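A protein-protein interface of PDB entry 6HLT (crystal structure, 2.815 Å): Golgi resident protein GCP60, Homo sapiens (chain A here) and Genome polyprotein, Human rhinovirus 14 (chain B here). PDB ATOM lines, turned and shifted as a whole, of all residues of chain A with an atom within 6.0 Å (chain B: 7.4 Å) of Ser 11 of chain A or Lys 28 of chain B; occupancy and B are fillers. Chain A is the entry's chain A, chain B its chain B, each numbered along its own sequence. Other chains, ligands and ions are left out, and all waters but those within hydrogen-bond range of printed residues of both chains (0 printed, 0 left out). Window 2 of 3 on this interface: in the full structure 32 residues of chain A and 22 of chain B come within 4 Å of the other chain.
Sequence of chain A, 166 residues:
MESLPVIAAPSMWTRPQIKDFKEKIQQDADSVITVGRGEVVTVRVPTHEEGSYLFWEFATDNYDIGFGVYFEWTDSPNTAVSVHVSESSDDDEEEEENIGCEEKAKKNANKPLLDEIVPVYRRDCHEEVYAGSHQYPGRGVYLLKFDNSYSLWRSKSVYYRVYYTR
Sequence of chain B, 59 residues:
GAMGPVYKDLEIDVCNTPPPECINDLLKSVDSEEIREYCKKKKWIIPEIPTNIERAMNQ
Among the printed residues, pairs that only touch across the chains: Trp 13 of chain A with Lys 28 of chain B, Trp 13 of chain A with Arg 36 of chain B, Trp 13 of chain A with Asn 24 of chain B and Ala 131 of chain A with Arg 36 of chain B.
The backbone carbonyl oxygen (O) of Ser 11 of chain A lies within hydrogen-bond range of the backbone NH (N) of Ser 133 of chain A, 2.8 Å away. The backbone carbonyl oxygen (O) of Trp 13 of chain A is in hydrogen-bond range of the backbone NH (N) of Ala 131 of chain A (3.0 Å). The side-chain carboxylate (OD1) of Asp 31 of chain B lies within salt-bridge range of the guanidinium group (NE) of Arg 36 of chain B.
Of the 12 printed residues of chain B, 5 touch a printed residue of chain A. Hydrophobic or aromatic side chains of chain B that line the printed part of chain A: Leu 27. Of the 11 printed residues of chain A, 4 touch a printed residue of chain B.
Lys 28 of chain B touches just these residues of chain A: Ser 11 and Trp 13. Of the printed residues of chain A, Asn 24 of chain B touches Ser 11, Trp 13 and Ser 133. Of the printed residues of chain A, Leu 27 of chain B touches Trp 13 (3.5 Å). The nearest printed residue of chain B that does not touch Ser 11 of chain A is Asp 25 of chain B (7.4 Å). The nearest residue of chain A that does not touch Lys 28 of chain B is Met 12 of chain A (5.2 Å).
OG of Ser 11 of chain A sits at hydrogen-bond distance from ND2 of Asn 24 of chain B (3.3 Å). The side-chain amino group (NZ) of Lys 28 of chain B sits at hydrogen-bond distance from the side-chain hydroxyl (OG) of Ser 11 of chain A (3.3 Å). NE1 of Trp 13 of chain A lies within hydrogen-bond range of O of Leu 27 of chain B (3.5 Å). OD2 of Asp 31 of chain B sits at hydrogen-bond distance from NE1 of Trp 13 of chain A. The side-chain amide oxygen (OD1) of Asn 24 of chain B sits at hydrogen-bond distance from the side-chain hydroxyl (OG) of Ser 133 of chain A (2.6 Å).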
ATOM      1  N   ALA A   9      10.690   6.520  13.251  1.00  0.00           N
ATOM      2  CA  ALA A   9      11.842   7.306  12.855  1.00  0.00           C
ATOM      3  C   ALA A   9      11.541   8.794  13.061  1.00  0.00           C
ATOM      4  O   ALA A   9      10.409   9.237  12.850  1.00  0.00           O
ATOM      5  CB  ALA A   9      12.211   7.014  11.409  1.00  0.00           C
ATOM      6  N   PRO A  10      12.551   9.565  13.501  1.00  0.00           N
ATOM      7  CA  PRO A  10      12.352  11.006  13.619  1.00  0.00           C
ATOM      8  C   PRO A  10      12.260  11.658  12.248  1.00  0.00           C
ATOM      9  O   PRO A  10      12.592  11.029  11.246  1.00  0.00           O
ATOM     10  CB  PRO A  10      13.603  11.469  14.370  1.00  0.00           C
ATOM     11  CG  PRO A  10      14.630  10.516  13.971  1.00  0.00           C
ATOM     12  CD  PRO A  10      13.935   9.189  13.843  1.00  0.00           C
ATOM     13  N   SER A  11      11.780  12.894  12.213  1.00  0.00           N
ATOM     14  CA  SER A  11      11.797  13.700  11.004  1.00  0.00           C
ATOM     15  C   SER A  11      12.674  14.921  11.262  1.00  0.00           C
ATOM     16  O   SER A  11      12.636  15.486  12.352  1.00  0.00           O
ATOM     17  CB  SER A  11      10.378  14.112  10.614  1.00  0.00           C
ATOM     18  OG  SER A  11       9.499  13.003  10.676  1.00  0.00           O
ATOM     19  N   MET A  12      13.477  15.310  10.277  1.00  0.00           N
ATOM     20  CA  MET A  12      14.327  16.491  10.409  1.00  0.00           C
ATOM     21  C   MET A  12      14.308  17.316   9.137  1.00  0.00           C
ATOM     22  O   MET A  12      14.107  16.794   8.043  1.00  0.00           O
ATOM     23  CB  MET A  12      15.767  16.100  10.748  1.00  0.00           C
ATOM     24  CG  MET A  12      15.953  15.570  12.171  1.00  0.00           C
ATOM     25  SD  MET A  12      17.547  16.008  12.896  1.00  0.00           S
ATOM     26  CE  MET A  12      17.391  17.791  13.099  1.00  0.00           C
ATOM     27  N   TRP A  13      14.515  18.617   9.292  1.00  0.00           N
ATOM     28  CA  TRP A  13      14.535  19.521   8.160  1.00  0.00           C
ATOM     29  C   TRP A  13      15.147  20.852   8.565  1.00  0.00           C
ATOM     30  O   TRP A  13      15.611  21.015   9.697  1.00  0.00           O
ATOM     31  CB  TRP A  13      13.124  19.728   7.614  1.00  0.00           C
ATOM     32  CG  TRP A  13      12.201  20.428   8.556  1.00  0.00           C
ATOM     33  CD1 TRP A  13      11.985  21.768   8.636  1.00  0.00           C
ATOM     34  CD2 TRP A  13      11.357  19.824   9.552  1.00  0.00           C
ATOM     35  NE1 TRP A  13      11.066  22.039   9.619  1.00  0.00           N
ATOM     36  CE2 TRP A  13      10.671  20.870  10.190  1.00  0.00           C
ATOM     37  CE3 TRP A  13      11.135  18.511   9.962  1.00  0.00           C
ATOM     38  CZ2 TRP A  13       9.764  20.630  11.219  1.00  0.00           C
ATOM     39  CZ3 TRP A  13      10.235  18.282  10.979  1.00  0.00           C
ATOM     40  CH2 TRP A  13       9.561  19.333  11.597  1.00  0.00           C
ATOM     41  N   THR A  14      15.155  21.801   7.636  1.00  0.00           N
ATOM     42  CA  THR A  14      15.672  23.134   7.914  1.00  0.00           C
ATOM     43  C   THR A  14      14.830  24.187   7.216  1.00  0.00           C
ATOM     44  O   THR A  14      14.152  23.899   6.230  1.00  0.00           O
ATOM     45  CB  THR A  14      17.136  23.279   7.466  1.00  0.00           C
ATOM     46  OG1 THR A  14      17.271  22.831   6.111  1.00  0.00           O
ATOM     47  CG2 THR A  14      18.040  22.451   8.353  1.00  0.00           C
ATOM     48  N   TRP A  56      11.170  20.073  17.881  1.00  0.00           N
ATOM     49  CA  TRP A  56      12.269  20.905  18.354  1.00  0.00           C
ATOM     50  C   TRP A  56      12.780  21.820  17.240  1.00  0.00           C
ATOM     51  O   TRP A  56      12.654  21.514  16.051  1.00  0.00           O
ATOM     52  CB  TRP A  56      13.415  20.032  18.902  1.00  0.00           C
ATOM     53  CG  TRP A  56      14.053  19.113  17.887  1.00  0.00           C
ATOM     54  CD1 TRP A  56      14.990  19.443  16.946  1.00  0.00           C
ATOM     55  CD2 TRP A  56      13.799  17.709  17.726  1.00  0.00           C
ATOM     56  NE1 TRP A  56      15.326  18.334  16.207  1.00  0.00           N
ATOM     57  CE2 TRP A  56      14.613  17.264  16.663  1.00  0.00           C
ATOM     58  CE3 TRP A  56      12.965  16.796  18.373  1.00  0.00           C
ATOM     59  CZ2 TRP A  56      14.605  15.938  16.236  1.00  0.00           C
ATOM     60  CZ3 TRP A  56      12.960  15.489  17.949  1.00  0.00           C
ATOM     61  CH2 TRP A  56      13.776  15.067  16.890  1.00  0.00           C
ATOM     62  N   ALA A 131      15.292  22.014  12.469  1.00  0.00           N
ATOM     63  CA  ALA A 131      14.074  21.554  13.113  1.00  0.00           C
ATOM     64  C   ALA A 131      13.945  20.049  12.997  1.00  0.00           C
ATOM     65  O   ALA A 131      14.651  19.400  12.226  1.00  0.00           O
ATOM     66  CB  ALA A 131      12.871  22.231  12.508  1.00  0.00           C
ATOM     67  N   GLY A 132      13.044  19.493  13.789  1.00  0.00           N
ATOM     68  CA  GLY A 132      12.797  18.073  13.743  1.00  0.00           C
ATOM     69  C   GLY A 132      11.625  17.708  14.619  1.00  0.00           C
ATOM     70  O   GLY A 132      11.138  18.520  15.407  1.00  0.00           O
ATOM     71  N   SER A 133      11.174  16.471  14.476  1.00  0.00           N
ATOM     72  CA  SER A 133      10.055  15.972  15.252  1.00  0.00           C
ATOM     73  C   SER A 133      10.213  14.483  15.505  1.00  0.00           C
ATOM     74  O   SER A 133      10.918  13.792  14.774  1.00  0.00           O
ATOM     75  CB  SER A 133       8.739  16.237  14.521  1.00  0.00           C
ATOM     76  OG  SER A 133       8.651  15.438  13.355  1.00  0.00           O
ATOM     77  N   HIS A 134       9.562  13.992  16.554  1.00  0.00           N
ATOM     78  CA  HIS A 134       9.504  12.552  16.777  1.00  0.00           C
ATOM     79  C   HIS A 134       8.233  12.170  17.531  1.00  0.00           C
ATOM     80  O   HIS A 134       7.746  12.925  18.368  1.00  0.00           O
ATOM     81  CB  HIS A 134      10.748  12.091  17.548  1.00  0.00           C
ATOM     82  CG  HIS A 134      10.841  10.603  17.687  1.00  0.00           C
ATOM     83  ND1 HIS A 134      10.653   9.960  18.892  1.00  0.00           N
ATOM     84  CD2 HIS A 134      11.096   9.636  16.781  1.00  0.00           C
ATOM     85  CE1 HIS A 134      10.795   8.658  18.717  1.00  0.00           C
ATOM     86  NE2 HIS A 134      11.064   8.436  17.443  1.00  0.00           N
ATOM     87  N   GLU B  21       0.179  13.598  12.604  1.00  0.00           N
ATOM     88  CA  GLU B  21       1.014  13.249  11.458  1.00  0.00           C
ATOM     89  C   GLU B  21       0.947  14.301  10.346  1.00  0.00           C
ATOM     90  O   GLU B  21       1.912  14.481   9.599  1.00  0.00           O
ATOM     91  CB  GLU B  21       0.605  11.882  10.904  1.00  0.00           C
ATOM     92  N   CYS B  22      -0.192  14.984  10.231  1.00  0.00           N
ATOM     93  CA  CYS B  22      -0.386  15.993   9.186  1.00  0.00           C
ATOM     94  C   CYS B  22       0.222  17.340   9.560  1.00  0.00           C
ATOM     95  O   CYS B  22       0.646  18.102   8.694  1.00  0.00           O
ATOM     96  CB  CYS B  22      -1.877  16.173   8.868  1.00  0.00           C
ATOM     97  SG  CYS B  22      -2.663  14.731   8.085  1.00  0.00           S
ATOM     98  N   ILE B  23       0.244  17.637  10.854  1.00  0.00           N
ATOM     99  CA  ILE B  23       0.878  18.854  11.344  1.00  0.00           C
ATOM    100  C   ILE B  23       2.360  18.819  11.009  1.00  0.00           C
ATOM    101  O   ILE B  23       2.993  19.856  10.803  1.00  0.00           O
ATOM    102  CB  ILE B  23       0.699  19.011  12.856  1.00  0.00           C
ATOM    103  CG1 ILE B  23      -0.788  19.085  13.200  1.00  0.00           C
ATOM    104  CG2 ILE B  23       1.390  20.268  13.342  1.00  0.00           C
ATOM    105  CD1 ILE B  23      -1.089  18.903  14.666  1.00  0.00           C
ATOM    106  N   ASN B  24       2.898  17.607  10.949  1.00  0.00           N
ATOM    107  CA  ASN B  24       4.309  17.413  10.670  1.00  0.00           C
ATOM    108  C   ASN B  24       4.663  17.623   9.200  1.00  0.00           C
ATOM    109  O   ASN B  24       5.680  18.246   8.896  1.00  0.00           O
ATOM    110  CB  ASN B  24       4.743  16.015  11.114  1.00  0.00           C
ATOM    111  CG  ASN B  24       6.244  15.849  11.104  1.00  0.00           C
ATOM    112  OD1 ASN B  24       6.967  16.620  11.734  1.00  0.00           O
ATOM    113  ND2 ASN B  24       6.723  14.848  10.382  1.00  0.00           N
ATOM    114  N   ASP B  25       3.835  17.107   8.293  1.00  0.00           N
ATOM    115  CA  ASP B  25       4.096  17.244   6.858  1.00  0.00           C
ATOM    116  C   ASP B  25       4.059  18.712   6.451  1.00  0.00           C
ATOM    117  O   ASP B  25       4.814  19.151   5.577  1.00  0.00           O
ATOM    118  CB  ASP B  25       3.083  16.445   6.035  1.00  0.00           C
ATOM    119  CG  ASP B  25       3.465  16.352   4.560  1.00  0.00           C
ATOM    120  OD1 ASP B  25       3.205  17.314   3.800  1.00  0.00           O
ATOM    121  OD2 ASP B  25       4.020  15.309   4.155  1.00  0.00           O
ATOM    122  N   LEU B  26       3.165  19.462   7.085  1.00  0.00           N
ATOM    123  CA  LEU B  26       3.069  20.890   6.847  1.00  0.00           C
ATOM    124  C   LEU B  26       4.387  21.585   7.164  1.00  0.00           C
ATOM    125  O   LEU B  26       5.034  22.130   6.270  1.00  0.00           O
ATOM    126  CB  LEU B  26       1.938  21.490   7.678  1.00  0.00           C
ATOM    127  CG  LEU B  26       1.762  23.005   7.560  1.00  0.00           C
ATOM    128  CD1 LEU B  26       1.409  23.423   6.131  1.00  0.00           C
ATOM    129  CD2 LEU B  26       0.709  23.468   8.538  1.00  0.00           C
ATOM    130  N   LEU B  27       4.769  21.559   8.440  1.00  0.00           N
ATOM    131  CA  LEU B  27       5.965  22.247   8.927  1.00  0.00           C
ATOM    132  C   LEU B  27       7.229  21.825   8.156  1.00  0.00           C
ATOM    133  O   LEU B  27       8.098  22.657   7.900  1.00  0.00           O
ATOM    134  CB  LEU B  27       6.135  22.003  10.438  1.00  0.00           C
ATOM    135  CG  LEU B  27       5.054  22.651  11.336  1.00  0.00           C
ATOM    136  CD1 LEU B  27       5.061  22.108  12.756  1.00  0.00           C
ATOM    137  CD2 LEU B  27       5.185  24.171  11.395  1.00  0.00           C
ATOM    138  N   LYS B  28       7.321  20.555   7.763  1.00  0.00           N
ATOM    139  CA  LYS B  28       8.422  20.115   6.903  1.00  0.00           C
ATOM    140  C   LYS B  28       8.471  20.959   5.640  1.00  0.00           C
ATOM    141  O   LYS B  28       9.491  21.585   5.331  1.00  0.00           O
ATOM    142  CB  LYS B  28       8.270  18.645   6.506  1.00  0.00           C
ATOM    143  CG  LYS B  28       8.618  17.657   7.598  1.00  0.00           C
ATOM    144  CD  LYS B  28       9.076  16.324   7.023  1.00  0.00           C
ATOM    145  CE  LYS B  28       8.547  15.162   7.849  1.00  0.00           C
ATOM    146  NZ  LYS B  28       9.203  13.869   7.495  1.00  0.00           N
ATOM    147  N   SER B  29       7.346  20.961   4.927  1.00  0.00           N
ATOM    148  CA  SER B  29       7.233  21.571   3.606  1.00  0.00           C
ATOM    149  C   SER B  29       7.217  23.093   3.663  1.00  0.00           C
ATOM    150  O   SER B  29       7.950  23.758   2.934  1.00  0.00           O
ATOM    151  CB  SER B  29       5.971  21.065   2.912  1.00  0.00           C
ATOM    152  OG  SER B  29       5.922  19.648   2.908  1.00  0.00           O
ATOM    153  N   VAL B  30       6.366  23.638   4.522  1.00  0.00           N
ATOM    154  CA  VAL B  30       6.285  25.083   4.714  1.00  0.00           C
ATOM    155  C   VAL B  30       6.518  25.423   6.178  1.00  0.00           C
ATOM    156  O   VAL B  30       5.696  25.100   7.032  1.00  0.00           O
ATOM    157  CB  VAL B  30       4.915  25.640   4.287  1.00  0.00           C
ATOM    158  CG1 VAL B  30       4.859  27.133   4.540  1.00  0.00           C
ATOM    159  CG2 VAL B  30       4.655  25.333   2.825  1.00  0.00           C
ATOM    160  N   ASP B  31       7.625  26.101   6.457  1.00  0.00           N
ATOM    161  CA  ASP B  31       8.010  26.399   7.829  1.00  0.00           C
ATOM    162  C   ASP B  31       8.384  27.860   7.929  1.00  0.00           C
ATOM    163  O   ASP B  31       9.206  28.360   7.161  1.00  0.00           O
ATOM    164  CB  ASP B  31       9.186  25.518   8.282  1.00  0.00           C
ATOM    165  CG  ASP B  31       9.121  25.145   9.765  1.00  0.00           C
ATOM    166  OD1 ASP B  31       8.550  25.899  10.584  1.00  0.00           O
ATOM    167  OD2 ASP B  31       9.661  24.083  10.115  1.00  0.00           O
ATOM    168  N   ARG B  36       4.221  28.650  12.567  1.00  0.00           N
ATOM    169  CA  ARG B  36       4.405  28.257  13.955  1.00  0.00           C
ATOM    170  C   ARG B  36       3.398  28.973  14.856  1.00  0.00           C
ATOM    171  O   ARG B  36       2.734  28.342  15.676  1.00  0.00           O
ATOM    172  CB  ARG B  36       5.840  28.544  14.405  1.00  0.00           C
ATOM    173  CG  ARG B  36       6.897  27.692  13.701  1.00  0.00           C
ATOM    174  CD  ARG B  36       6.992  26.298  14.298  1.00  0.00           C
ATOM    175  NE  ARG B  36       7.915  25.439  13.556  1.00  0.00           N
ATOM    176  CZ  ARG B  36       8.407  24.292  14.018  1.00  0.00           C
ATOM    177  NH1 ARG B  36       8.080  23.868  15.231  1.00  0.00           N
ATOM    178  NH2 ARG B  36       9.242  23.575  13.276  1.00  0.00           N
